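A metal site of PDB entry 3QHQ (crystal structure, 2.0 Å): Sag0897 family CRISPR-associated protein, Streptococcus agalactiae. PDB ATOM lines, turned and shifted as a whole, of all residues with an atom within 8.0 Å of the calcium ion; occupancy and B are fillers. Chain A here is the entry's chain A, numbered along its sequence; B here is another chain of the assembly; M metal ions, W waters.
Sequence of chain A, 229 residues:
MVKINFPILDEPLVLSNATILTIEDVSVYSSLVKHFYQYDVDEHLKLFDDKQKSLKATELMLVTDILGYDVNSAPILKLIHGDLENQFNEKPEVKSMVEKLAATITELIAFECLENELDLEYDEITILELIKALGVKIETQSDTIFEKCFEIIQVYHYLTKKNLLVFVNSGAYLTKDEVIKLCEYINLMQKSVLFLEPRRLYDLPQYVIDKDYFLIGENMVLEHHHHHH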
ATOM      1  N   ALA A 110      14.418  21.611  17.142  1.00  0.00           N
ATOM      2  CA  ALA A 110      13.821  21.592  18.487  1.00  0.00           C
ATOM      3  C   ALA A 110      13.939  22.954  19.167  1.00  0.00           C
ATOM      4  O   ALA A 110      12.998  23.405  19.835  1.00  0.00           O
ATOM      5  CB  ALA A 110      14.462  20.518  19.358  1.00  0.00           C
ATOM      6  N   PHE A 111      15.084  23.605  18.999  1.00  0.00           N
ATOM      7  CA  PHE A 111      15.280  24.945  19.565  1.00  0.00           C
ATOM      8  C   PHE A 111      14.287  25.942  18.984  1.00  0.00           C
ATOM      9  O   PHE A 111      13.704  26.728  19.728  1.00  0.00           O
ATOM     10  CB  PHE A 111      16.727  25.427  19.381  1.00  0.00           C
ATOM     11  CG  PHE A 111      17.031  26.705  20.121  1.00  0.00           C
ATOM     12  CD1 PHE A 111      17.086  27.918  19.455  1.00  0.00           C
ATOM     13  CD2 PHE A 111      17.228  26.686  21.507  1.00  0.00           C
ATOM     14  CE1 PHE A 111      17.353  29.100  20.149  1.00  0.00           C
ATOM     15  CE2 PHE A 111      17.496  27.860  22.206  1.00  0.00           C
ATOM     16  CZ  PHE A 111      17.551  29.077  21.527  1.00  0.00           C
ATOM     17  N   GLU A 112      14.103  25.907  17.663  1.00  0.00           N
ATOM     18  CA  GLU A 112      13.130  26.782  17.002  1.00  0.00           C
ATOM     19  C   GLU A 112      11.691  26.512  17.451  1.00  0.00           C
ATOM     20  O   GLU A 112      10.890  27.435  17.542  1.00  0.00           O
ATOM     21  CB  GLU A 112      13.246  26.708  15.480  1.00  0.00           C
ATOM     22  CG  GLU A 112      14.583  27.178  14.909  1.00  0.00           C
ATOM     23  CD  GLU A 112      14.991  28.577  15.382  1.00  0.00           C
ATOM     24  OE1 GLU A 112      14.132  29.484  15.451  1.00  0.00           O
ATOM     25  OE2 GLU A 112      16.191  28.764  15.676  1.00  0.00           O
ATOM     26  N   CYS A 113      11.394  25.239  17.727  1.00  0.00           N
ATOM     27  CA  CYS A 113      10.089  24.845  18.272  1.00  0.00           C
ATOM     28  C   CYS A 113       9.822  25.479  19.644  1.00  0.00           C
ATOM     29  O   CYS A 113       8.720  25.959  19.897  1.00  0.00           O
ATOM     30  CB  CYS A 113       9.947  23.326  18.358  1.00  0.00           C
ATOM     31  SG  CYS A 113       9.726  22.504  16.768  1.00  0.00           S
ATOM     32  N   LEU A 114      10.831  25.477  20.516  1.00  0.00           N
ATOM     33  CA  LEU A 114      10.735  26.128  21.823  1.00  0.00           C
ATOM     34  C   LEU A 114      10.658  27.660  21.711  1.00  0.00           C
ATOM     35  O   LEU A 114       9.951  28.285  22.478  1.00  0.00           O
ATOM     36  CB  LEU A 114      11.877  25.724  22.758  1.00  0.00           C
ATOM     37  CG  LEU A 114      11.852  24.308  23.365  1.00  0.00           C
ATOM     38  CD1 LEU A 114      13.197  24.002  24.013  1.00  0.00           C
ATOM     39  CD2 LEU A 114      10.712  24.157  24.386  1.00  0.00           C
ATOM     40  N   GLU A 115      11.371  28.232  20.748  1.00  0.00           N
ATOM     41  CA  GLU A 115      11.285  29.677  20.487  1.00  0.00           C
ATOM     42  C   GLU A 115       9.888  30.067  19.970  1.00  0.00           C
ATOM     43  O   GLU A 115       9.364  31.114  20.341  1.00  0.00           O
ATOM     44  CB  GLU A 115      12.359  30.131  19.488  1.00  0.00           C
ATOM     45  CG  GLU A 115      13.792  29.966  19.992  1.00  0.00           C
ATOM     46  CD  GLU A 115      14.205  31.055  20.974  1.00  0.00           C
ATOM     47  OE1 GLU A 115      13.997  30.885  22.191  1.00  0.00           O
ATOM     48  OE2 GLU A 115      14.766  32.064  20.533  1.00  0.00           O
ATOM     49  N   ASN A 116       9.293  29.206  19.137  1.00  0.00           N
ATOM     50  CA  ASN A 116       7.929  29.385  18.647  1.00  0.00           C
ATOM     51  C   ASN A 116       6.918  29.493  19.798  1.00  0.00           C
ATOM     52  O   ASN A 116       7.061  28.798  20.808  1.00  0.00           O
ATOM     53  CB  ASN A 116       7.535  28.220  17.731  1.00  0.00           C
ATOM     54  CG  ASN A 116       6.313  28.530  16.893  1.00  0.00           C
ATOM     55  OD1 ASN A 116       5.188  28.446  17.366  1.00  0.00           O
ATOM     56  ND2 ASN A 116       6.544  28.894  15.632  1.00  0.00           N
ATOM     57  N   GLU A 117       5.917  30.355  19.643  1.00  0.00           N
ATOM     58  CA  GLU A 117       4.943  30.603  20.713  1.00  0.00           C
ATOM     59  C   GLU A 117       3.990  29.436  20.967  1.00  0.00           C
ATOM     60  O   GLU A 117       3.414  29.338  22.060  1.00  0.00           O
ATOM     61  CB  GLU A 117       4.156  31.883  20.432  1.00  0.00           C
ATOM     62  CG  GLU A 117       3.296  31.828  19.188  1.00  0.00           C
ATOM     63  CD  GLU A 117       2.403  33.037  19.056  1.00  0.00           C
ATOM     64  OE1 GLU A 117       2.918  34.179  19.177  1.00  0.00           O
ATOM     65  OE2 GLU A 117       1.192  32.850  18.828  1.00  0.00           O
ATOM     66  N   LEU A 118       3.812  28.559  19.984  1.00  0.00           N
ATOM     67  CA  LEU A 118       2.979  27.368  20.165  1.00  0.00           C
ATOM     68  C   LEU A 118       3.705  26.322  20.986  1.00  0.00           C
ATOM     69  O   LEU A 118       4.926  26.227  20.943  1.00  0.00           O
ATOM     70  CB  LEU A 118       2.590  26.758  18.815  1.00  0.00           C
ATOM     71  CG  LEU A 118       1.386  27.364  18.095  1.00  0.00           C
ATOM     72  CD1 LEU A 118       1.449  27.006  16.615  1.00  0.00           C
ATOM     73  CD2 LEU A 118       0.078  26.899  18.723  1.00  0.00           C
ATOM     74  N   ASP A 119       2.932  25.537  21.747  1.00  0.00           N
ATOM     75  CA  ASP A 119       3.476  24.399  22.467  1.00  0.00           C
ATOM     76  C   ASP A 119       3.629  23.236  21.500  1.00  0.00           C
ATOM     77  O   ASP A 119       2.657  22.555  21.148  1.00  0.00           O
ATOM     78  CB  ASP A 119       2.585  24.036  23.647  1.00  0.00           C
ATOM     79  CG  ASP A 119       3.076  22.821  24.401  1.00  0.00           C
ATOM     80  OD1 ASP A 119       4.317  22.646  24.518  1.00  0.00           O
ATOM     81  OD2 ASP A 119       2.243  22.035  24.856  1.00  0.00           O
ATOM     82  N   LEU A 120       4.860  23.021  21.054  1.00  0.00           N
ATOM     83  CA  LEU A 120       5.129  22.090  19.967  1.00  0.00           C
ATOM     84  C   LEU A 120       5.840  20.827  20.435  1.00  0.00           C
ATOM     85  O   LEU A 120       6.675  20.860  21.344  1.00  0.00           O
ATOM     86  CB  LEU A 120       5.937  22.782  18.862  1.00  0.00           C
ATOM     87  CG  LEU A 120       5.269  23.962  18.147  1.00  0.00           C
ATOM     88  CD1 LEU A 120       6.255  24.641  17.211  1.00  0.00           C
ATOM     89  CD2 LEU A 120       4.002  23.516  17.388  1.00  0.00           C
ATOM     90  N   GLU A 121       5.480  19.729  19.807  1.00  0.00           N
ATOM     91  CA  GLU A 121       6.144  18.446  19.993  1.00  0.00           C
ATOM     92  C   GLU A 121       6.490  17.869  18.624  1.00  0.00           C
ATOM     93  O   GLU A 121       6.100  18.441  17.589  1.00  0.00           O
ATOM     94  CB  GLU A 121       5.262  17.483  20.799  1.00  0.00           C
ATOM     95  CG  GLU A 121       3.985  17.031  20.076  1.00  0.00           C
ATOM     96  CD  GLU A 121       3.204  15.995  20.856  1.00  0.00           C
ATOM     97  OE1 GLU A 121       3.763  15.407  21.809  1.00  0.00           O
ATOM     98  OE2 GLU A 121       2.027  15.757  20.523  1.00  0.00           O
ATOM     99  N   LEU B  84       8.126  27.989  11.021  1.00  0.00           N
ATOM    100  CA  LEU B  84       9.405  27.494  11.531  1.00  0.00           C
ATOM    101  C   LEU B  84      10.558  27.636  10.529  1.00  0.00           C
ATOM    102  O   LEU B  84      11.677  27.982  10.910  1.00  0.00           O
ATOM    103  CB  LEU B  84       9.279  26.032  11.978  1.00  0.00           C
ATOM    104  CG  LEU B  84       8.532  25.790  13.286  1.00  0.00           C
ATOM    105  CD1 LEU B  84       8.279  24.302  13.454  1.00  0.00           C
ATOM    106  CD2 LEU B  84       9.288  26.338  14.491  1.00  0.00           C
ATOM    107  N   GLN B  87      11.658  31.198  10.668  1.00  0.00           N
ATOM    108  CA  GLN B  87      12.527  31.418  11.825  1.00  0.00           C
ATOM    109  C   GLN B  87      14.000  31.107  11.498  1.00  0.00           C
ATOM    110  O   GLN B  87      14.898  31.832  11.919  1.00  0.00           O
ATOM    111  CB  GLN B  87      12.062  30.596  13.025  1.00  0.00           C
ATOM    112  CG  GLN B  87      10.811  31.131  13.708  1.00  0.00           C
ATOM    113  CD  GLN B  87      10.277  30.212  14.790  1.00  0.00           C
ATOM    114  OE1 GLN B  87       9.073  30.119  14.993  1.00  0.00           O
ATOM    115  NE2 GLN B  87      11.168  29.536  15.505  1.00  0.00           N
ATOM    116  N   GLN B 154      -4.091  30.736  18.981  1.00  0.00           N
ATOM    117  CA  GLN B 154      -2.814  30.833  18.259  1.00  0.00           C
ATOM    118  C   GLN B 154      -2.924  30.304  16.824  1.00  0.00           C
ATOM    119  O   GLN B 154      -2.300  30.824  15.911  1.00  0.00           O
ATOM    120  CB  GLN B 154      -1.706  30.117  19.014  1.00  0.00           C
ATOM    121  CG  GLN B 154      -1.281  30.789  20.312  1.00  0.00           C
ATOM    122  CD  GLN B 154      -0.270  29.966  21.088  1.00  0.00           C
ATOM    123  OE1 GLN B 154      -0.554  28.841  21.493  1.00  0.00           O
ATOM    124  NE2 GLN B 154       0.906  30.531  21.291  1.00  0.00           N
HETATM  125 CA    CA M   1       7.162  26.516  21.578  1.00  0.00          CA
HETATM  126  O   HOH W   1       7.299  24.292  22.412  1.00  0.00           O
HETATM  127  O   HOH W   2       7.595  27.306  24.174  1.00  0.00           O
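The backbone NH of Leu 118 lies within hydrogen-bond range of the side-chain amide oxygen of Asn 116 (3.0 Å). The side-chain amide nitrogen (ND2) of Asn 116 lies within hydrogen-bond range of the side-chain amide oxygen (OE1) of Gln 87 of chain B.
Residues that only touch the calcium ion: Leu 114 (3.4 Å). Four residues have an atom within 4 Å of the calcium ion: Cys 113, Leu 114, Asn 116 and Leu 118. The nearest printed residue that does not touch the calcium ion is Leu 120 (4.2 Å).
The calcium ion is bound by O of Leu 118 (2.3 Å), O of Cys 113 (2.4 Å), water W1 (2.4 Å), O of Asn 116 (2.4 Å) and water W2 (2.7 Å). The calcium ion has five donor atoms within binding distance.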
